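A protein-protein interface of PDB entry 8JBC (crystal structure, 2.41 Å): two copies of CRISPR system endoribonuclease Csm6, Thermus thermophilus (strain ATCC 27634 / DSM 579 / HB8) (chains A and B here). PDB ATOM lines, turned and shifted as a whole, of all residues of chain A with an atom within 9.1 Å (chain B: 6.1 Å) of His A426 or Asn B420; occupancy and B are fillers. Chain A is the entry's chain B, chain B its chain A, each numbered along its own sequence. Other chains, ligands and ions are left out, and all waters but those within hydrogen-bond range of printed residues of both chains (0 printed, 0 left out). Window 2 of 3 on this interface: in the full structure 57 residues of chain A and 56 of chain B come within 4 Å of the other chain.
The guanidinium group of Arg B333 lies within hydrogen-bond range of the backbone carbonyl oxygen of Leu A423, at 2.8 Å. The guanidinium group (NH2) of Arg A333 sits at hydrogen-bond distance from the backbone carbonyl oxygen (O) of Gly B427, 2.6 Å away. The guanidinium group (NH2) of Arg B333 sits at hydrogen-bond distance from the backbone carbonyl oxygen (O) of Gly A427 (2.7 Å). The guanidinium group of Arg A419 lies within hydrogen-bond range of the backbone carbonyl oxygen of Val B425 (2.6 Å). The backbone carbonyl oxygen of Val A425 sits at hydrogen-bond distance from the guanidinium group of Arg B419, at 2.6 Å. The side-chain carboxylate (OD1) of Asp B429 lies within salt-bridge range of the guanidinium group (NH1) of Arg A297, 3.2 Å away. The guanidinium group (NH2) of Arg B333 lies within hydrogen-bond range of the backbone carbonyl oxygen (O) of His A426. The backbone carbonyl oxygen (O) of Val A425 sits close to the side-chain carboxylate (OE1) of Glu B336 (3.4 Å). The side-chain amide oxygen (OD1) of Asn B420 lies within hydrogen-bond range of a ring nitrogen (NE2) of His A426 (3.2 Å). The backbone carbonyl oxygen of Leu B423 sits at hydrogen-bond distance from the guanidinium group of Arg A333, 3.0 Å away. The side-chain amide oxygen (OD1) of Asn A420 sits at hydrogen-bond distance from a ring nitrogen (NE2) of His B426. The backbone carbonyl oxygen (O) of His B426 lies within hydrogen-bond range of the guanidinium group (NH2) of Arg A333 (3.2 Å).
NH1 of Arg B333 lies within salt-bridge range of OE1 of Glu B336 (3.0 Å). The backbone carbonyl oxygen (O) of Ser B421 is in hydrogen-bond range of the backbone NH (N) of Phe B428 (2.9 Å). The guanidinium group (NH2) of Arg B419 lies within salt-bridge range of the side-chain carboxylate (OE1) of Glu B336 (2.4 Å). The backbone NH (N) of Asp B429 lies within hydrogen-bond range of the backbone carbonyl oxygen (O) of Ser B421 (2.9 Å). N of Leu B423 is in hydrogen-bond range of O of Asp B429, at 3.4 Å. The backbone NH (N) of His A426 sits at hydrogen-bond distance from the backbone carbonyl oxygen (O) of Asn A420 (3.1 Å).
Among the printed residues, merely in contact across the chains: Val A425 with Arg B333 (3.3 Å), His A426 with Glu B336 (3.4 Å), Arg A297 with Phe B428 (3.5 Å), His A426 with Arg B419 (3.6 Å), Arg A333 with Val B425 (3.6 Å), Arg A333 with Phe B428 (3.6 Å), Glu A336 with Val B425 (3.7 Å), Glu A336 with His B426 (3.7 Å), Arg A419 with His B426 (3.7 Å), Phe A428 with Arg B333 (3.9 Å) and His A426 with His B426 (3.98 Å).
Of the printed residues of chain B, Glu A336 touches Val B425 and His B426. Gly A418 touches none of the printed residues of chain B. Ser A421 touches none of the printed residues of chain B. Of the printed residues of chain B, His A426 touches Arg B333, Glu B336, Arg B419, Asn B420 and His B426. Printed residues of chain B within 4 Å of Phe A428: Arg B333. No residue of chain A comes within 4 Å of Gly B418. Printed residues of chain A within 4 Å of Arg B419: Val A425 (2.6 Å) and His A426 (3.6 Å). No residue of chain A comes within 4 Å of Ser B421. No residue of chain A comes within 4 Å of Ala B422. Of the printed residues of chain A, Leu B423 touches Arg A333. Printed residues of chain A within 4 Å of His B426: Arg A333 (3.2 Å), Glu A336 (3.7 Å), Arg A419 (3.7 Å), Asn A420 (2.9 Å) and His A426 (3.98 Å). The nearest printed residue of chain B that does not touch His A426 is Val B425 (4.7 Å). The nearest residue of chain A that does not touch Asn B420 is Val A425 (6.0 Å).
Along chain B the printed residues that touch a printed residue of chain A span positions 333 to 429. Among the printed residues, 23 pairs touch across the chains.
Arg A333 touches Leu B423, and with the chains exchanged Leu A423 touches Arg B333. Arg A333 touches Val B425, and with the chains exchanged Val A425 touches Arg B333. Glu A336 touches His B426, and with the chains exchanged His A426 touches Glu B336. His A426 touches its own counterpart, His B426. Of the 23 pairs that touch across the chains among the printed residues, 21 have their exchanged pair printed and touching as well.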
ATOM      1  N   ARG A 297      -7.777 -16.441  -0.702  1.00  0.00           N
ATOM      2  CA  ARG A 297      -6.989 -15.602   0.214  1.00  0.00           C
ATOM      3  C   ARG A 297      -5.487 -15.707  -0.052  1.00  0.00           C
ATOM      4  O   ARG A 297      -4.673 -15.650   0.870  1.00  0.00           O
ATOM      5  CB  ARG A 297      -7.308 -15.927   1.670  1.00  0.00           C
ATOM      6  CG  ARG A 297      -8.777 -16.176   1.870  1.00  0.00           C
ATOM      7  CD  ARG A 297      -9.195 -16.185   3.326  1.00  0.00           C
ATOM      8  NE  ARG A 297     -10.387 -17.011   3.495  1.00  0.00           N
ATOM      9  CZ  ARG A 297     -11.366 -16.762   4.358  1.00  0.00           C
ATOM     10  NH1 ARG A 297     -11.359 -15.675   5.121  1.00  0.00           N
ATOM     11  NH2 ARG A 297     -12.384 -17.620   4.450  1.00  0.00           N
ATOM     12  N   LEU A 329     -11.695   3.770   8.009  1.00  0.00           N
ATOM     13  CA  LEU A 329     -11.740   2.315   8.027  1.00  0.00           C
ATOM     14  C   LEU A 329     -11.526   1.708   6.641  1.00  0.00           C
ATOM     15  O   LEU A 329     -10.799   0.721   6.498  1.00  0.00           O
ATOM     16  CB  LEU A 329     -13.073   1.860   8.587  1.00  0.00           C
ATOM     17  CG  LEU A 329     -13.092   0.353   8.537  1.00  0.00           C
ATOM     18  CD1 LEU A 329     -12.766  -0.159   9.904  1.00  0.00           C
ATOM     19  CD2 LEU A 329     -14.436  -0.073   8.037  1.00  0.00           C
ATOM     20  N   ARG A 333      -7.983  -0.525   5.360  1.00  0.00           N
ATOM     21  CA  ARG A 333      -8.019  -1.870   4.802  1.00  0.00           C
ATOM     22  C   ARG A 333      -7.391  -1.912   3.406  1.00  0.00           C
ATOM     23  O   ARG A 333      -6.679  -2.864   3.064  1.00  0.00           O
ATOM     24  CB  ARG A 333      -9.459  -2.386   4.779  1.00  0.00           C
ATOM     25  CG  ARG A 333      -9.576  -3.885   4.454  1.00  0.00           C
ATOM     26  CD  ARG A 333      -8.842  -4.708   5.498  1.00  0.00           C
ATOM     27  NE  ARG A 333      -9.076  -6.135   5.306  1.00  0.00           N
ATOM     28  CZ  ARG A 333      -8.122  -7.016   5.047  1.00  0.00           C
ATOM     29  NH1 ARG A 333      -6.843  -6.666   5.035  1.00  0.00           N
ATOM     30  NH2 ARG A 333      -8.462  -8.272   4.762  1.00  0.00           N
ATOM     31  N   GLU A 336      -3.697  -1.642   3.774  1.00  0.00           N
ATOM     32  CA  GLU A 336      -3.209  -2.869   4.380  1.00  0.00           C
ATOM     33  C   GLU A 336      -3.031  -3.949   3.328  1.00  0.00           C
ATOM     34  O   GLU A 336      -1.945  -4.517   3.200  1.00  0.00           O
ATOM     35  CB  GLU A 336      -4.156  -3.310   5.485  1.00  0.00           C
ATOM     36  CG  GLU A 336      -3.642  -4.456   6.332  1.00  0.00           C
ATOM     37  CD  GLU A 336      -4.575  -4.776   7.488  1.00  0.00           C
ATOM     38  OE1 GLU A 336      -5.712  -5.231   7.244  1.00  0.00           O
ATOM     39  OE2 GLU A 336      -4.171  -4.543   8.649  1.00  0.00           O
ATOM     40  N   GLY A 418      -2.137   4.531  13.732  1.00  0.00           N
ATOM     41  CA  GLY A 418      -3.503   4.472  14.201  1.00  0.00           C
ATOM     42  C   GLY A 418      -4.378   3.418  13.559  1.00  0.00           C
ATOM     43  O   GLY A 418      -5.595   3.447  13.780  1.00  0.00           O
ATOM     44  N   ARG A 419      -3.802   2.468  12.810  1.00  0.00           N
ATOM     45  CA  ARG A 419      -4.592   1.514  12.022  1.00  0.00           C
ATOM     46  C   ARG A 419      -5.584   0.717  12.874  1.00  0.00           C
ATOM     47  O   ARG A 419      -6.685   0.387  12.412  1.00  0.00           O
ATOM     48  CB  ARG A 419      -3.660   0.554  11.285  1.00  0.00           C
ATOM     49  CG  ARG A 419      -4.353  -0.396  10.307  1.00  0.00           C
ATOM     50  CD  ARG A 419      -4.675  -1.768  10.897  1.00  0.00           C
ATOM     51  NE  ARG A 419      -5.409  -2.582   9.935  1.00  0.00           N
ATOM     52  CZ  ARG A 419      -6.687  -2.413   9.618  1.00  0.00           C
ATOM     53  NH1 ARG A 419      -7.433  -1.485  10.205  1.00  0.00           N
ATOM     54  NH2 ARG A 419      -7.236  -3.203   8.701  1.00  0.00           N
ATOM     55  N   ASN A 420      -5.197   0.339  14.091  1.00  0.00           N
ATOM     56  CA  ASN A 420      -6.069  -0.468  14.944  1.00  0.00           C
ATOM     57  C   ASN A 420      -6.716   0.337  16.050  1.00  0.00           C
ATOM     58  O   ASN A 420      -7.696  -0.131  16.647  1.00  0.00           O
ATOM     59  CB  ASN A 420      -5.300  -1.654  15.544  1.00  0.00           C
ATOM     60  CG  ASN A 420      -5.043  -2.751  14.511  1.00  0.00           C
ATOM     61  OD1 ASN A 420      -5.970  -3.205  13.829  1.00  0.00           O
ATOM     62  ND2 ASN A 420      -3.770  -3.125  14.338  1.00  0.00           N
ATOM     63  N   SER A 421      -6.226   1.545  16.302  1.00  0.00           N
ATOM     64  CA  SER A 421      -6.837   2.441  17.268  1.00  0.00           C
ATOM     65  C   SER A 421      -7.993   3.240  16.670  1.00  0.00           C
ATOM     66  O   SER A 421      -8.645   4.006  17.391  1.00  0.00           O
ATOM     67  CB  SER A 421      -5.763   3.370  17.843  1.00  0.00           C
ATOM     68  OG  SER A 421      -5.261   4.236  16.846  1.00  0.00           O
ATOM     69  N   ALA A 422      -8.275   3.058  15.385  1.00  0.00           N
ATOM     70  CA  ALA A 422      -9.461   3.650  14.798  1.00  0.00           C
ATOM     71  C   ALA A 422     -10.711   3.152  15.523  1.00  0.00           C
ATOM     72  O   ALA A 422     -10.726   2.078  16.118  1.00  0.00           O
ATOM     73  CB  ALA A 422      -9.521   3.313  13.316  1.00  0.00           C
ATOM     74  N   LEU A 423     -11.761   3.969  15.495  1.00  0.00           N
ATOM     75  CA  LEU A 423     -12.916   3.732  16.348  1.00  0.00           C
ATOM     76  C   LEU A 423     -13.684   2.484  15.930  1.00  0.00           C
ATOM     77  O   LEU A 423     -14.241   1.785  16.774  1.00  0.00           O
ATOM     78  CB  LEU A 423     -13.827   4.955  16.325  1.00  0.00           C
ATOM     79  CG  LEU A 423     -15.213   4.757  16.925  1.00  0.00           C
ATOM     80  CD1 LEU A 423     -15.097   4.467  18.417  1.00  0.00           C
ATOM     81  CD2 LEU A 423     -16.026   5.988  16.695  1.00  0.00           C
ATOM     82  N   LEU A 424     -13.715   2.179  14.648  1.00  0.00           N
ATOM     83  CA  LEU A 424     -14.442   1.025  14.160  1.00  0.00           C
ATOM     84  C   LEU A 424     -13.577  -0.222  14.077  1.00  0.00           C
ATOM     85  O   LEU A 424     -13.998  -1.206  13.465  1.00  0.00           O
ATOM     86  CB  LEU A 424     -15.047   1.328  12.785  1.00  0.00           C
ATOM     87  CG  LEU A 424     -16.245   2.274  12.823  1.00  0.00           C
ATOM     88  CD1 LEU A 424     -16.585   2.723  11.415  1.00  0.00           C
ATOM     89  CD2 LEU A 424     -17.432   1.620  13.518  1.00  0.00           C
ATOM     90  N   VAL A 425     -12.373  -0.205  14.644  1.00  0.00           N
ATOM     91  CA  VAL A 425     -11.625  -1.452  14.756  1.00  0.00           C
ATOM     92  C   VAL A 425     -11.497  -1.842  16.222  1.00  0.00           C
ATOM     93  O   VAL A 425     -12.313  -2.625  16.714  1.00  0.00           O
ATOM     94  CB  VAL A 425     -10.248  -1.304  14.088  1.00  0.00           C
ATOM     95  CG1 VAL A 425      -9.389  -2.524  14.315  1.00  0.00           C
ATOM     96  CG2 VAL A 425     -10.423  -1.004  12.606  1.00  0.00           C
ATOM     97  N   HIS A 426     -10.608  -1.186  16.981  1.00  0.00           N
ATOM     98  CA  HIS A 426     -10.398  -1.572  18.383  1.00  0.00           C
ATOM     99  C   HIS A 426     -10.245  -0.384  19.318  1.00  0.00           C
ATOM    100  O   HIS A 426     -10.073  -0.595  20.520  1.00  0.00           O
ATOM    101  CB  HIS A 426      -9.152  -2.473  18.557  1.00  0.00           C
ATOM    102  CG  HIS A 426      -9.230  -3.774  17.822  1.00  0.00           C
ATOM    103  ND1 HIS A 426      -8.165  -4.294  17.116  1.00  0.00           N
ATOM    104  CD2 HIS A 426     -10.244  -4.663  17.681  1.00  0.00           C
ATOM    105  CE1 HIS A 426      -8.523  -5.438  16.557  1.00  0.00           C
ATOM    106  NE2 HIS A 426      -9.781  -5.684  16.885  1.00  0.00           N
ATOM    107  N   GLY A 427     -10.281   0.848  18.816  1.00  0.00           N
ATOM    108  CA  GLY A 427      -9.979   2.006  19.621  1.00  0.00           C
ATOM    109  C   GLY A 427     -11.058   3.071  19.531  1.00  0.00           C
ATOM    110  O   GLY A 427     -12.259   2.794  19.367  1.00  0.00           O
ATOM    111  N   PHE A 428     -10.607   4.310  19.664  1.00  0.00           N
ATOM    112  CA  PHE A 428     -11.522   5.412  19.898  1.00  0.00           C
ATOM    113  C   PHE A 428     -11.122   6.642  19.104  1.00  0.00           C
ATOM    114  O   PHE A 428     -11.623   7.735  19.385  1.00  0.00           O
ATOM    115  CB  PHE A 428     -11.577   5.743  21.394  1.00  0.00           C
ATOM    116  CG  PHE A 428     -11.857   4.555  22.265  1.00  0.00           C
ATOM    117  CD1 PHE A 428     -10.822   3.726  22.686  1.00  0.00           C
ATOM    118  CD2 PHE A 428     -13.155   4.277  22.694  1.00  0.00           C
ATOM    119  CE1 PHE A 428     -11.080   2.633  23.497  1.00  0.00           C
ATOM    120  CE2 PHE A 428     -13.414   3.193  23.524  1.00  0.00           C
ATOM    121  CZ  PHE A 428     -12.374   2.370  23.925  1.00  0.00           C
ATOM    122  N   ASP A 429     -10.236   6.503  18.136  1.00  0.00           N
ATOM    123  CA  ASP A 429      -9.758   7.659  17.402  1.00  0.00           C
ATOM    124  C   ASP A 429     -10.839   8.190  16.481  1.00  0.00           C
ATOM    125  O   ASP A 429     -11.415   7.447  15.681  1.00  0.00           O
ATOM    126  CB  ASP A 429      -8.528   7.287  16.588  1.00  0.00           C
ATOM    127  CG  ASP A 429      -7.393   6.818  17.454  1.00  0.00           C
ATOM    128  OD1 ASP A 429      -7.471   7.014  18.696  1.00  0.00           O
ATOM    129  OD2 ASP A 429      -6.448   6.214  16.895  1.00  0.00           O
ATOM    130  N   TYR B 332     -20.028  -5.890  15.722  1.00  0.00           N
ATOM    131  CA  TYR B 332     -18.850  -6.362  16.448  1.00  0.00           C
ATOM    132  C   TYR B 332     -18.323  -5.295  17.399  1.00  0.00           C
ATOM    133  O   TYR B 332     -18.084  -5.565  18.588  1.00  0.00           O
ATOM    134  CB  TYR B 332     -17.753  -6.764  15.460  1.00  0.00           C
ATOM    135  CG  TYR B 332     -17.868  -8.172  14.893  1.00  0.00           C
ATOM    136  CD1 TYR B 332     -17.984  -9.294  15.731  1.00  0.00           C
ATOM    137  CD2 TYR B 332     -17.854  -8.379  13.516  1.00  0.00           C
ATOM    138  CE1 TYR B 332     -18.086 -10.590  15.193  1.00  0.00           C
ATOM    139  CE2 TYR B 332     -17.954  -9.647  12.975  1.00  0.00           C
ATOM    140  CZ  TYR B 332     -18.072 -10.751  13.815  1.00  0.00           C
ATOM    141  OH  TYR B 332     -18.161 -11.998  13.243  1.00  0.00           O
ATOM    142  N   ARG B 333     -18.150  -4.064  16.895  1.00  0.00           N
ATOM    143  CA  ARG B 333     -17.571  -3.018  17.731  1.00  0.00           C
ATOM    144  C   ARG B 333     -18.479  -2.692  18.906  1.00  0.00           C
ATOM    145  O   ARG B 333     -17.998  -2.300  19.979  1.00  0.00           O
ATOM    146  CB  ARG B 333     -17.284  -1.761  16.896  1.00  0.00           C
ATOM    147  CG  ARG B 333     -16.462  -0.694  17.652  1.00  0.00           C
ATOM    148  CD  ARG B 333     -15.032  -1.182  17.941  1.00  0.00           C
ATOM    149  NE  ARG B 333     -14.282  -0.211  18.724  1.00  0.00           N
ATOM    150  CZ  ARG B 333     -13.876  -0.382  19.974  1.00  0.00           C
ATOM    151  NH1 ARG B 333     -14.133  -1.498  20.645  1.00  0.00           N
ATOM    152  NH2 ARG B 333     -13.208   0.596  20.572  1.00  0.00           N
ATOM    153  N   GLU B 336     -18.035  -5.784  21.388  1.00  0.00           N
ATOM    154  CA  GLU B 336     -16.732  -5.689  22.032  1.00  0.00           C
ATOM    155  C   GLU B 336     -16.750  -4.657  23.148  1.00  0.00           C
ATOM    156  O   GLU B 336     -16.177  -4.876  24.220  1.00  0.00           O
ATOM    157  CB  GLU B 336     -15.685  -5.338  20.979  1.00  0.00           C
ATOM    158  CG  GLU B 336     -14.244  -5.300  21.438  1.00  0.00           C
ATOM    159  CD  GLU B 336     -13.277  -5.109  20.262  1.00  0.00           C
ATOM    160  OE1 GLU B 336     -13.456  -4.138  19.495  1.00  0.00           O
ATOM    161  OE2 GLU B 336     -12.344  -5.920  20.086  1.00  0.00           O
ATOM    162  N   GLN B 340     -16.430  -5.454  27.267  1.00  0.00           N
ATOM    163  CA  GLN B 340     -15.364  -4.792  28.004  1.00  0.00           C
ATOM    164  C   GLN B 340     -15.900  -3.900  29.102  1.00  0.00           C
ATOM    165  O   GLN B 340     -15.182  -3.637  30.074  1.00  0.00           O
ATOM    166  CB  GLN B 340     -14.482  -3.983  27.050  1.00  0.00           C
ATOM    167  CG  GLN B 340     -13.646  -4.855  26.131  1.00  0.00           C
ATOM    168  CD  GLN B 340     -12.678  -4.064  25.272  1.00  0.00           C
ATOM    169  OE1 GLN B 340     -12.079  -3.082  25.719  1.00  0.00           O
ATOM    170  NE2 GLN B 340     -12.503  -4.507  24.032  1.00  0.00           N
ATOM    171  N   LYS B 417     -16.091 -15.371  16.808  1.00  0.00           N
ATOM    172  CA  LYS B 417     -14.651 -15.440  16.640  1.00  0.00           C
ATOM    173  C   LYS B 417     -14.192 -14.867  15.309  1.00  0.00           C
ATOM    174  O   LYS B 417     -12.983 -14.842  15.052  1.00  0.00           O
ATOM    175  CB  LYS B 417     -14.164 -16.889  16.777  1.00  0.00           C
ATOM    176  CG  LYS B 417     -14.732 -17.781  15.694  1.00  0.00           C
ATOM    177  CD  LYS B 417     -13.731 -18.772  15.156  1.00  0.00           C
ATOM    178  CE  LYS B 417     -14.199 -19.257  13.790  1.00  0.00           C
ATOM    179  NZ  LYS B 417     -15.087 -20.467  13.876  1.00  0.00           N
ATOM    180  N   GLY B 418     -15.116 -14.426  14.457  1.00  0.00           N
ATOM    181  CA  GLY B 418     -14.763 -13.771  13.213  1.00  0.00           C
ATOM    182  C   GLY B 418     -14.627 -12.270  13.387  1.00  0.00           C
ATOM    183  O   GLY B 418     -14.643 -11.518  12.414  1.00  0.00           O
ATOM    184  N   ARG B 419     -14.485 -11.841  14.642  1.00  0.00           N
ATOM    185  CA  ARG B 419     -14.395 -10.424  14.966  1.00  0.00           C
ATOM    186  C   ARG B 419     -13.293  -9.739  14.185  1.00  0.00           C
ATOM    187  O   ARG B 419     -13.437  -8.575  13.794  1.00  0.00           O
ATOM    188  CB  ARG B 419     -14.144 -10.234  16.455  1.00  0.00           C
ATOM    189  CG  ARG B 419     -14.308  -8.801  16.900  1.00  0.00           C
ATOM    190  CD  ARG B 419     -12.982  -8.054  16.968  1.00  0.00           C
ATOM    191  NE  ARG B 419     -13.192  -6.679  17.401  1.00  0.00           N
ATOM    192  CZ  ARG B 419     -13.772  -5.750  16.652  1.00  0.00           C
ATOM    193  NH1 ARG B 419     -14.123  -5.992  15.399  1.00  0.00           N
ATOM    194  NH2 ARG B 419     -14.032  -4.560  17.179  1.00  0.00           N
ATOM    195  N   ASN B 420     -12.173 -10.433  13.970  1.00  0.00           N
ATOM    196  CA  ASN B 420     -11.074  -9.852  13.220  1.00  0.00           C
ATOM    197  C   ASN B 420     -10.983 -10.362  11.795  1.00  0.00           C
ATOM    198  O   ASN B 420     -10.374  -9.691  10.951  1.00  0.00           O
ATOM    199  CB  ASN B 420      -9.745 -10.089  13.940  1.00  0.00           C
ATOM    200  CG  ASN B 420      -9.692  -9.378  15.285  1.00  0.00           C
ATOM    201  OD1 ASN B 420      -8.965  -8.404  15.460  1.00  0.00           O
ATOM    202  ND2 ASN B 420     -10.466  -9.867  16.240  1.00  0.00           N
ATOM    203  N   SER B 421     -11.612 -11.484  11.493  1.00  0.00           N
ATOM    204  CA  SER B 421     -11.593 -12.036  10.149  1.00  0.00           C
ATOM    205  C   SER B 421     -12.597 -11.358   9.227  1.00  0.00           C
ATOM    206  O   SER B 421     -12.658 -11.692   8.034  1.00  0.00           O
ATOM    207  CB  SER B 421     -11.907 -13.522  10.243  1.00  0.00           C
ATOM    208  OG  SER B 421     -11.761 -13.937  11.589  1.00  0.00           O
ATOM    209  N   ALA B 422     -13.418 -10.465   9.772  1.00  0.00           N
ATOM    210  CA  ALA B 422     -14.283  -9.602   8.979  1.00  0.00           C
ATOM    211  C   ALA B 422     -13.523  -8.963   7.822  1.00  0.00           C
ATOM    212  O   ALA B 422     -12.380  -8.531   7.978  1.00  0.00           O
ATOM    213  CB  ALA B 422     -14.862  -8.517   9.881  1.00  0.00           C
ATOM    214  N   LEU B 423     -14.172  -8.910   6.654  1.00  0.00           N
ATOM    215  CA  LEU B 423     -13.571  -8.262   5.492  1.00  0.00           C
ATOM    216  C   LEU B 423     -13.068  -6.848   5.811  1.00  0.00           C
ATOM    217  O   LEU B 423     -12.020  -6.426   5.307  1.00  0.00           O
ATOM    218  CB  LEU B 423     -14.571  -8.201   4.334  1.00  0.00           C
ATOM    219  CG  LEU B 423     -14.026  -7.407   3.142  1.00  0.00           C
ATOM    220  CD1 LEU B 423     -12.757  -8.095   2.682  1.00  0.00           C
ATOM    221  CD2 LEU B 423     -15.036  -7.243   1.959  1.00  0.00           C
ATOM    222  N   VAL B 425     -12.067  -5.687   8.760  1.00  0.00           N
ATOM    223  CA  VAL B 425     -11.131  -5.519   9.864  1.00  0.00           C
ATOM    224  C   VAL B 425      -9.757  -6.022   9.440  1.00  0.00           C
ATOM    225  O   VAL B 425      -8.883  -5.227   9.079  1.00  0.00           O
ATOM    226  CB  VAL B 425     -11.633  -6.249  11.131  1.00  0.00           C
ATOM    227  CG1 VAL B 425     -10.637  -6.088  12.289  1.00  0.00           C
ATOM    228  CG2 VAL B 425     -13.049  -5.768  11.535  1.00  0.00           C
ATOM    229  N   HIS B 426      -9.596  -7.344   9.353  1.00  0.00           N
ATOM    230  CA  HIS B 426      -8.291  -7.927   9.038  1.00  0.00           C
ATOM    231  C   HIS B 426      -8.358  -9.066   8.045  1.00  0.00           C
ATOM    232  O   HIS B 426      -7.314  -9.433   7.499  1.00  0.00           O
ATOM    233  CB  HIS B 426      -7.603  -8.433  10.308  1.00  0.00           C
ATOM    234  CG  HIS B 426      -7.145  -7.348  11.224  1.00  0.00           C
ATOM    235  ND1 HIS B 426      -7.151  -7.486  12.597  1.00  0.00           N
ATOM    236  CD2 HIS B 426      -6.645  -6.117  10.973  1.00  0.00           C
ATOM    237  CE1 HIS B 426      -6.680  -6.384  13.153  1.00  0.00           C
ATOM    238  NE2 HIS B 426      -6.369  -5.535  12.188  1.00  0.00           N
ATOM    239  N   GLY B 427      -9.532  -9.632   7.781  1.00  0.00           N
ATOM    240  CA  GLY B 427      -9.659 -10.839   6.996  1.00  0.00           C
ATOM    241  C   GLY B 427     -10.565 -10.678   5.801  1.00  0.00           C
ATOM    242  O   GLY B 427     -10.593  -9.612   5.179  1.00  0.00           O
ATOM    243  N   PHE B 428     -11.324 -11.727   5.482  1.00  0.00           N
ATOM    244  CA  PHE B 428     -11.993 -11.813   4.190  1.00  0.00           C
ATOM    245  C   PHE B 428     -13.412 -12.345   4.316  1.00  0.00           C
ATOM    246  O   PHE B 428     -14.005 -12.764   3.309  1.00  0.00           O
ATOM    247  CB  PHE B 428     -11.165 -12.682   3.241  1.00  0.00           C
ATOM    248  CG  PHE B 428      -9.795 -12.161   3.031  1.00  0.00           C
ATOM    249  CD1 PHE B 428      -9.567 -11.116   2.132  1.00  0.00           C
ATOM    250  CD2 PHE B 428      -8.729 -12.657   3.761  1.00  0.00           C
ATOM    251  CE1 PHE B 428      -8.293 -10.589   1.951  1.00  0.00           C
ATOM    252  CE2 PHE B 428      -7.439 -12.149   3.579  1.00  0.00           C
ATOM    253  CZ  PHE B 428      -7.222 -11.109   2.676  1.00  0.00           C
ATOM    254  N   ASP B 429     -13.976 -12.309   5.511  1.00  0.00           N
ATOM    255  CA  ASP B 429     -15.263 -12.945   5.744  1.00  0.00           C
ATOM    256  C   ASP B 429     -16.388 -12.143   5.106  1.00  0.00           C
ATOM    257  O   ASP B 429     -16.602 -10.972   5.449  1.00  0.00           O
ATOM    258  CB  ASP B 429     -15.501 -13.101   7.246  1.00  0.00           C
ATOM    259  CG  ASP B 429     -14.510 -14.037   7.893  1.00  0.00           C
ATOM    260  OD1 ASP B 429     -13.641 -14.580   7.151  1.00  0.00           O
ATOM    261  OD2 ASP B 429     -14.592 -14.213   9.139  1.00  0.00           O
